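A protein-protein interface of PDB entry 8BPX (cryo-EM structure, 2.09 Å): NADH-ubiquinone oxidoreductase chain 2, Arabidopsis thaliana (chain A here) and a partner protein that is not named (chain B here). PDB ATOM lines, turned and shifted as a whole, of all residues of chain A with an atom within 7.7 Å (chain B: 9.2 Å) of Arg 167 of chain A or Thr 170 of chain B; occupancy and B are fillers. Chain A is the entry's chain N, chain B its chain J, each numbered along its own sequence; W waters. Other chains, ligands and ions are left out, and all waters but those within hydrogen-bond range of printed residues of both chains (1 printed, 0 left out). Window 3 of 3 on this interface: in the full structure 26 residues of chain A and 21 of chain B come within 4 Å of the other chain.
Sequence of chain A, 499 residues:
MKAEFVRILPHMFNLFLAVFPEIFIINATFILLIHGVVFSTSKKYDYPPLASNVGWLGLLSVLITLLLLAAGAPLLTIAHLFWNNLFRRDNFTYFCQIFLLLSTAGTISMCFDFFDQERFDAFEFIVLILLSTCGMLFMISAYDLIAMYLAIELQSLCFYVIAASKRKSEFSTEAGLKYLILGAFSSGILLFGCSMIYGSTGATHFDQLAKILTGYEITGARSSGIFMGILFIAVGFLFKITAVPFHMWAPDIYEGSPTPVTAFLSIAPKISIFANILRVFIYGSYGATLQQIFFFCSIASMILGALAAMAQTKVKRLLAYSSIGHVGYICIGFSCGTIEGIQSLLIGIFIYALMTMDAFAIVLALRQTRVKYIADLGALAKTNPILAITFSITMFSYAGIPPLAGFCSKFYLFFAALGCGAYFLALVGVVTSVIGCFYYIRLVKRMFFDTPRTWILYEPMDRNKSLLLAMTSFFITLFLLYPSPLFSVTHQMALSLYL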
ATOM      1  N   PHE A 120     -13.565 -10.654 -10.917  1.00  0.00           N
ATOM      2  CA  PHE A 120     -13.360 -10.977 -12.322  1.00  0.00           C
ATOM      3  C   PHE A 120     -12.559 -12.277 -12.340  1.00  0.00           C
ATOM      4  O   PHE A 120     -11.340 -12.264 -12.168  1.00  0.00           O
ATOM      5  CB  PHE A 120     -12.637  -9.832 -13.024  1.00  0.00           C
ATOM      6  CG  PHE A 120     -12.570  -9.969 -14.511  1.00  0.00           C
ATOM      7  CD1 PHE A 120     -11.580 -10.733 -15.105  1.00  0.00           C
ATOM      8  CD2 PHE A 120     -13.489  -9.324 -15.318  1.00  0.00           C
ATOM      9  CE1 PHE A 120     -11.513 -10.857 -16.477  1.00  0.00           C
ATOM     10  CE2 PHE A 120     -13.427  -9.443 -16.690  1.00  0.00           C
ATOM     11  CZ  PHE A 120     -12.436 -10.210 -17.270  1.00  0.00           C
ATOM     12  N   VAL A 161     -11.282  -8.284 -28.015  1.00  0.00           N
ATOM     13  CA  VAL A 161     -11.895  -9.230 -27.086  1.00  0.00           C
ATOM     14  C   VAL A 161     -11.835  -8.711 -25.652  1.00  0.00           C
ATOM     15  O   VAL A 161     -12.828  -8.780 -24.919  1.00  0.00           O
ATOM     16  CB  VAL A 161     -11.253 -10.621 -27.216  1.00  0.00           C
ATOM     17  CG1 VAL A 161     -11.793 -11.545 -26.137  1.00  0.00           C
ATOM     18  CG2 VAL A 161     -11.528 -11.194 -28.592  1.00  0.00           C
ATOM     19  N   ALA A 163     -11.523  -5.609 -24.466  1.00  0.00           N
ATOM     20  CA  ALA A 163     -12.387  -4.406 -24.302  1.00  0.00           C
ATOM     21  C   ALA A 163     -13.854  -4.808 -23.978  1.00  0.00           C
ATOM     22  O   ALA A 163     -14.499  -4.088 -23.271  1.00  0.00           O
ATOM     23  CB  ALA A 163     -12.331  -3.446 -25.463  1.00  0.00           C
ATOM     24  N   ALA A 164     -14.309  -5.941 -24.466  1.00  0.00           N
ATOM     25  CA  ALA A 164     -15.672  -6.393 -24.230  1.00  0.00           C
ATOM     26  C   ALA A 164     -15.757  -7.447 -23.130  1.00  0.00           C
ATOM     27  O   ALA A 164     -16.741  -8.191 -23.074  1.00  0.00           O
ATOM     28  CB  ALA A 164     -16.276  -6.933 -25.527  1.00  0.00           C
ATOM     29  N   SER A 165     -14.748  -7.522 -22.255  1.00  0.00           N
ATOM     30  CA  SER A 165     -14.674  -8.621 -21.294  1.00  0.00           C
ATOM     31  C   SER A 165     -15.817  -8.584 -20.285  1.00  0.00           C
ATOM     32  O   SER A 165     -16.283  -9.642 -19.848  1.00  0.00           O
ATOM     33  CB  SER A 165     -13.324  -8.615 -20.574  1.00  0.00           C
ATOM     34  OG  SER A 165     -12.914  -7.301 -20.245  1.00  0.00           O
ATOM     35  N   LYS A 166     -16.242  -7.379 -19.876  1.00  0.00           N
ATOM     36  CA  LYS A 166     -17.464  -7.273 -19.025  1.00  0.00           C
ATOM     37  C   LYS A 166     -18.610  -7.413 -20.022  1.00  0.00           C
ATOM     38  O   LYS A 166     -19.157  -6.388 -20.453  1.00  0.00           O
ATOM     39  CB  LYS A 166     -17.457  -5.987 -18.192  1.00  0.00           C
ATOM     40  CG  LYS A 166     -16.349  -5.915 -17.149  1.00  0.00           C
ATOM     41  CD  LYS A 166     -16.850  -5.685 -15.738  1.00  0.00           C
ATOM     42  CE  LYS A 166     -17.671  -6.837 -15.199  1.00  0.00           C
ATOM     43  NZ  LYS A 166     -18.099  -6.596 -13.801  1.00  0.00           N
ATOM     44  N   ARG A 167     -18.990  -8.646 -20.335  1.00  0.00           N
ATOM     45  CA  ARG A 167     -19.913  -8.917 -21.430  1.00  0.00           C
ATOM     46  C   ARG A 167     -21.382  -8.679 -21.080  1.00  0.00           C
ATOM     47  O   ARG A 167     -22.213  -8.660 -21.992  1.00  0.00           O
ATOM     48  CB  ARG A 167     -19.706 -10.354 -21.918  1.00  0.00           C
ATOM     49  CG  ARG A 167     -20.240 -11.388 -20.966  1.00  0.00           C
ATOM     50  CD  ARG A 167     -19.668 -12.772 -21.186  1.00  0.00           C
ATOM     51  NE  ARG A 167     -20.391 -13.753 -20.387  1.00  0.00           N
ATOM     52  CZ  ARG A 167     -20.514 -15.038 -20.691  1.00  0.00           C
ATOM     53  NH1 ARG A 167     -19.931 -15.556 -21.761  1.00  0.00           N
ATOM     54  NH2 ARG A 167     -21.242 -15.823 -19.902  1.00  0.00           N
ATOM     55  N   LYS A 168     -21.727  -8.510 -19.804  1.00  0.00           N
ATOM     56  CA  LYS A 168     -23.063  -8.077 -19.402  1.00  0.00           C
ATOM     57  C   LYS A 168     -23.176  -6.576 -19.175  1.00  0.00           C
ATOM     58  O   LYS A 168     -24.273  -6.087 -18.897  1.00  0.00           O
ATOM     59  CB  LYS A 168     -23.513  -8.818 -18.137  1.00  0.00           C
ATOM     60  CG  LYS A 168     -23.543 -10.327 -18.266  1.00  0.00           C
ATOM     61  CD  LYS A 168     -24.304 -10.726 -19.523  1.00  0.00           C
ATOM     62  CE  LYS A 168     -23.520 -11.657 -20.415  1.00  0.00           C
ATOM     63  NZ  LYS A 168     -23.214 -12.955 -19.769  1.00  0.00           N
ATOM     64  N   SER A 169     -22.081  -5.832 -19.287  1.00  0.00           N
ATOM     65  CA  SER A 169     -22.114  -4.396 -19.073  1.00  0.00           C
ATOM     66  C   SER A 169     -22.466  -3.677 -20.370  1.00  0.00           C
ATOM     67  O   SER A 169     -21.953  -4.014 -21.440  1.00  0.00           O
ATOM     68  CB  SER A 169     -20.767  -3.898 -18.546  1.00  0.00           C
ATOM     69  OG  SER A 169     -20.554  -2.538 -18.881  1.00  0.00           O
ATOM     70  N   GLU A 170     -23.351  -2.685 -20.264  1.00  0.00           N
ATOM     71  CA  GLU A 170     -23.664  -1.854 -21.423  1.00  0.00           C
ATOM     72  C   GLU A 170     -22.424  -1.117 -21.916  1.00  0.00           C
ATOM     73  O   GLU A 170     -22.167  -1.051 -23.126  1.00  0.00           O
ATOM     74  CB  GLU A 170     -24.773  -0.860 -21.073  1.00  0.00           C
ATOM     75  CG  GLU A 170     -26.168  -1.465 -21.021  1.00  0.00           C
ATOM     76  CD  GLU A 170     -26.483  -2.096 -19.674  1.00  0.00           C
ATOM     77  OE1 GLU A 170     -25.683  -1.925 -18.731  1.00  0.00           O
ATOM     78  OE2 GLU A 170     -27.534  -2.763 -19.561  1.00  0.00           O
ATOM     79  N   SER A 172     -19.103  -1.806 -21.465  1.00  0.00           N
ATOM     80  CA  SER A 172     -18.064  -2.665 -22.032  1.00  0.00           C
ATOM     81  C   SER A 172     -18.456  -3.187 -23.412  1.00  0.00           C
ATOM     82  O   SER A 172     -17.631  -3.205 -24.334  1.00  0.00           O
ATOM     83  CB  SER A 172     -17.768  -3.820 -21.076  1.00  0.00           C
ATOM     84  OG  SER A 172     -16.678  -4.606 -21.520  1.00  0.00           O
ATOM     85  N   THR A 173     -19.714  -3.607 -23.576  1.00  0.00           N
ATOM     86  CA  THR A 173     -20.173  -4.065 -24.884  1.00  0.00           C
ATOM     87  C   THR A 173     -20.160  -2.932 -25.907  1.00  0.00           C
ATOM     88  O   THR A 173     -19.769  -3.137 -27.062  1.00  0.00           O
ATOM     89  CB  THR A 173     -21.570  -4.681 -24.774  1.00  0.00           C
ATOM     90  OG1 THR A 173     -22.458  -3.754 -24.139  1.00  0.00           O
ATOM     91  CG2 THR A 173     -21.525  -5.978 -23.971  1.00  0.00           C
ATOM     92  N   PRO A 258     -12.948  -2.262 -19.168  1.00  0.00           N
ATOM     93  CA  PRO A 258     -12.493  -2.441 -17.782  1.00  0.00           C
ATOM     94  C   PRO A 258     -11.181  -1.708 -17.554  1.00  0.00           C
ATOM     95  O   PRO A 258     -10.292  -1.712 -18.406  1.00  0.00           O
ATOM     96  CB  PRO A 258     -12.327  -3.959 -17.651  1.00  0.00           C
ATOM     97  CG  PRO A 258     -13.169  -4.536 -18.724  1.00  0.00           C
ATOM     98  CD  PRO A 258     -13.182  -3.547 -19.847  1.00  0.00           C
ATOM     99  N   VAL B  68     -26.346 -15.732 -37.896  1.00  0.00           N
ATOM    100  CA  VAL B  68     -26.519 -14.680 -36.899  1.00  0.00           C
ATOM    101  C   VAL B  68     -27.667 -13.751 -37.285  1.00  0.00           C
ATOM    102  O   VAL B  68     -28.549 -13.460 -36.470  1.00  0.00           O
ATOM    103  CB  VAL B  68     -25.205 -13.907 -36.696  1.00  0.00           C
ATOM    104  CG1 VAL B  68     -25.463 -12.621 -35.931  1.00  0.00           C
ATOM    105  CG2 VAL B  68     -24.204 -14.776 -35.956  1.00  0.00           C
ATOM    106  N   ALA B 162      -9.358 -15.939 -32.080  1.00  0.00           N
ATOM    107  CA  ALA B 162     -10.768 -15.951 -32.467  1.00  0.00           C
ATOM    108  C   ALA B 162     -11.550 -16.997 -31.677  1.00  0.00           C
ATOM    109  O   ALA B 162     -12.642 -16.719 -31.170  1.00  0.00           O
ATOM    110  CB  ALA B 162     -10.909 -16.200 -33.969  1.00  0.00           C
ATOM    111  N   MET B 163     -10.997 -18.207 -31.557  1.00  0.00           N
ATOM    112  CA  MET B 163     -11.683 -19.272 -30.823  1.00  0.00           C
ATOM    113  C   MET B 163     -11.899 -18.886 -29.361  1.00  0.00           C
ATOM    114  O   MET B 163     -13.017 -18.993 -28.825  1.00  0.00           O
ATOM    115  CB  MET B 163     -10.880 -20.573 -30.924  1.00  0.00           C
ATOM    116  CG  MET B 163     -10.394 -20.872 -32.329  1.00  0.00           C
ATOM    117  SD  MET B 163      -9.212 -22.222 -32.506  1.00  0.00           S
ATOM    118  CE  MET B 163     -10.150 -23.611 -31.909  1.00  0.00           C
ATOM    119  N   ILE B 164     -10.836 -18.413 -28.706  1.00  0.00           N
ATOM    120  CA  ILE B 164     -10.932 -18.048 -27.295  1.00  0.00           C
ATOM    121  C   ILE B 164     -11.957 -16.939 -27.101  1.00  0.00           C
ATOM    122  O   ILE B 164     -12.801 -17.003 -26.199  1.00  0.00           O
ATOM    123  CB  ILE B 164      -9.554 -17.639 -26.746  1.00  0.00           C
ATOM    124  CG1 ILE B 164      -8.642 -18.859 -26.608  1.00  0.00           C
ATOM    125  CG2 ILE B 164      -9.706 -16.921 -25.411  1.00  0.00           C
ATOM    126  CD1 ILE B 164      -7.216 -18.508 -26.247  1.00  0.00           C
ATOM    127  N   GLY B 165     -11.893 -15.903 -27.941  1.00  0.00           N
ATOM    128  CA  GLY B 165     -12.816 -14.789 -27.805  1.00  0.00           C
ATOM    129  C   GLY B 165     -14.260 -15.194 -28.019  1.00  0.00           C
ATOM    130  O   GLY B 165     -15.149 -14.775 -27.271  1.00  0.00           O
ATOM    131  N   ALA B 166     -14.511 -16.026 -29.035  1.00  0.00           N
ATOM    132  CA  ALA B 166     -15.862 -16.519 -29.268  1.00  0.00           C
ATOM    133  C   ALA B 166     -16.401 -17.235 -28.039  1.00  0.00           C
ATOM    134  O   ALA B 166     -17.553 -17.023 -27.646  1.00  0.00           O
ATOM    135  CB  ALA B 166     -15.888 -17.447 -30.481  1.00  0.00           C
ATOM    136  N   ILE B 167     -15.582 -18.082 -27.411  1.00  0.00           N
ATOM    137  CA  ILE B 167     -16.058 -18.767 -26.210  1.00  0.00           C
ATOM    138  C   ILE B 167     -16.306 -17.770 -25.077  1.00  0.00           C
ATOM    139  O   ILE B 167     -17.393 -17.736 -24.493  1.00  0.00           O
ATOM    140  CB  ILE B 167     -15.081 -19.874 -25.780  1.00  0.00           C
ATOM    141  CG1 ILE B 167     -15.075 -21.016 -26.799  1.00  0.00           C
ATOM    142  CG2 ILE B 167     -15.457 -20.385 -24.394  1.00  0.00           C
ATOM    143  CD1 ILE B 167     -16.448 -21.459 -27.245  1.00  0.00           C
ATOM    144  N   VAL B 168     -15.316 -16.927 -24.770  1.00  0.00           N
ATOM    145  CA  VAL B 168     -15.404 -16.108 -23.561  1.00  0.00           C
ATOM    146  C   VAL B 168     -16.537 -15.095 -23.655  1.00  0.00           C
ATOM    147  O   VAL B 168     -17.145 -14.744 -22.639  1.00  0.00           O
ATOM    148  CB  VAL B 168     -14.065 -15.405 -23.255  1.00  0.00           C
ATOM    149  CG1 VAL B 168     -12.959 -16.422 -23.045  1.00  0.00           C
ATOM    150  CG2 VAL B 168     -13.702 -14.416 -24.352  1.00  0.00           C
ATOM    151  N   LEU B 169     -16.852 -14.608 -24.856  1.00  0.00           N
ATOM    152  CA  LEU B 169     -17.856 -13.555 -24.940  1.00  0.00           C
ATOM    153  C   LEU B 169     -19.284 -14.092 -24.979  1.00  0.00           C
ATOM    154  O   LEU B 169     -20.191 -13.432 -24.467  1.00  0.00           O
ATOM    155  CB  LEU B 169     -17.579 -12.669 -26.153  1.00  0.00           C
ATOM    156  CG  LEU B 169     -16.228 -11.948 -26.067  1.00  0.00           C
ATOM    157  CD1 LEU B 169     -15.679 -11.602 -27.440  1.00  0.00           C
ATOM    158  CD2 LEU B 169     -16.329 -10.712 -25.182  1.00  0.00           C
ATOM    159  N   THR B 170     -19.515 -15.279 -25.544  1.00  0.00           N
ATOM    160  CA  THR B 170     -20.879 -15.730 -25.794  1.00  0.00           C
ATOM    161  C   THR B 170     -21.313 -16.968 -25.017  1.00  0.00           C
ATOM    162  O   THR B 170     -22.520 -17.206 -24.922  1.00  0.00           O
ATOM    163  CB  THR B 170     -21.090 -16.008 -27.293  1.00  0.00           C
ATOM    164  OG1 THR B 170     -20.238 -17.078 -27.712  1.00  0.00           O
ATOM    165  CG2 THR B 170     -20.782 -14.762 -28.119  1.00  0.00           C
ATOM    166  N   MET B 171     -20.390 -17.749 -24.461  1.00  0.00           N
ATOM    167  CA  MET B 171     -20.751 -19.034 -23.869  1.00  0.00           C
ATOM    168  C   MET B 171     -21.631 -18.862 -22.634  1.00  0.00           C
ATOM    169  O   MET B 171     -21.300 -18.109 -21.716  1.00  0.00           O
ATOM    170  CB  MET B 171     -19.491 -19.818 -23.502  1.00  0.00           C
ATOM    171  CG  MET B 171     -19.743 -21.204 -22.923  1.00  0.00           C
ATOM    172  SD  MET B 171     -21.179 -22.040 -23.624  1.00  0.00           S
ATOM    173  CE  MET B 171     -20.369 -23.272 -24.636  1.00  0.00           C
ATOM    174  N   HIS B 172     -22.753 -19.580 -22.621  1.00  0.00           N
ATOM    175  CA  HIS B 172     -23.607 -19.748 -21.444  1.00  0.00           C
ATOM    176  C   HIS B 172     -23.876 -21.248 -21.348  1.00  0.00           C
ATOM    177  O   HIS B 172     -24.776 -21.764 -22.014  1.00  0.00           O
ATOM    178  CB  HIS B 172     -24.902 -18.946 -21.557  1.00  0.00           C
ATOM    179  CG  HIS B 172     -24.727 -17.474 -21.357  1.00  0.00           C
ATOM    180  ND1 HIS B 172     -24.194 -16.649 -22.323  1.00  0.00           N
ATOM    181  CD2 HIS B 172     -25.016 -16.678 -20.301  1.00  0.00           C
ATOM    182  CE1 HIS B 172     -24.160 -15.409 -21.872  1.00  0.00           C
ATOM    183  NE2 HIS B 172     -24.651 -15.399 -20.646  1.00  0.00           N
ATOM    184  N   ARG B 173     -23.085 -21.946 -20.538  1.00  0.00           N
ATOM    185  CA  ARG B 173     -23.194 -23.397 -20.454  1.00  0.00           C
ATOM    186  C   ARG B 173     -24.459 -23.789 -19.699  1.00  0.00           C
ATOM    187  O   ARG B 173     -24.747 -23.251 -18.626  1.00  0.00           O
ATOM    188  CB  ARG B 173     -21.959 -23.984 -19.772  1.00  0.00           C
ATOM    189  CG  ARG B 173     -21.790 -25.486 -19.960  1.00  0.00           C
ATOM    190  CD  ARG B 173     -20.457 -25.971 -19.410  1.00  0.00           C
ATOM    191  NE  ARG B 173     -20.103 -27.294 -19.911  1.00  0.00           N
ATOM    192  CZ  ARG B 173     -18.870 -27.778 -19.941  1.00  0.00           C
ATOM    193  NH1 ARG B 173     -17.838 -27.074 -19.506  1.00  0.00           N
ATOM    194  NH2 ARG B 173     -18.664 -29.000 -20.424  1.00  0.00           N
HETATM  195  O   HOH W   1     -16.397 -11.523 -22.031  1.00  0.00           O
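The backbone carbonyl oxygen of Val 168 of chain B is in hydrogen-bond range of the guanidinium group of Arg 167 of chain A, at 3.0 Å. The backbone carbonyl oxygen (O) of Leu 169 of chain B lies close to the guanidinium group (NH1) of Arg 167 of chain A (3.4 Å). The backbone carbonyl oxygen of Met 171 of chain B sits at hydrogen-bond distance from the guanidinium group of Arg 167 of chain A (2.9 Å). NE2 of His 172 of chain B sits at hydrogen-bond distance from NZ of Lys 168 of chain A (3.0 Å).
The backbone carbonyl oxygen of Ala 166 of chain B lies within hydrogen-bond range of the side-chain hydroxyl of Thr 170 of chain B (2.7 Å). ND1 of His 172 of chain B is in hydrogen-bond range of O of Thr 170 of chain B (3.1 Å). The backbone NH of Arg 173 of chain B sits at hydrogen-bond distance from the side-chain sulfur of Met 171 of chain B (3.6 Å).
CG1 of Val 161 of chain A touches CA of Gly 165 of chain B, 3.8 Å away. Val 168 of chain B touches Val 161 of chain A. O of Ala 164 of chain A touches CD2 of Leu 169 of chain B (3.3 Å). Thr 170 of chain B touches Arg 167 of chain A. NH2 of Arg 167 of chain A touches NE2 of His 172 of chain B, 3.5 Å away.
Of the printed residues of chain A, Val 168 of chain B touches Val 161 and Arg 167. Of the printed residues of chain A, Leu 169 of chain B touches Ala 164 (3.3 Å) and Arg 167 (3.4 Å). Of chain A, only Arg 167 (3.8 Å) comes within 4 Å of Thr 170 of chain B. The nearest residue of chain A that does not touch Thr 170 of chain B is Lys 168 of chain A (6.7 Å).
Of the 13 printed residues of chain A, 4 touch a printed residue of chain B. Hydrophobic or aromatic side chains of chain A that line the printed part of chain B: Val 161 and Ala 164. Of the 13 printed residues of chain B, 6 touch a printed residue of chain A. Printed residues of chain B that touch a printed residue of chain A: Gly 165, Val 168, Leu 169, Thr 170, Met 171 and His 172. Among the printed residues, no Asp or Glu carboxylate lies within 4 Å of a Lys or Arg side-chain nitrogen of the other chain.
Water W1 lies within hydrogen-bond range of O of Ser 165 of chain A (2.9 Å) and O of Val 168 of chain B (3.4 Å).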
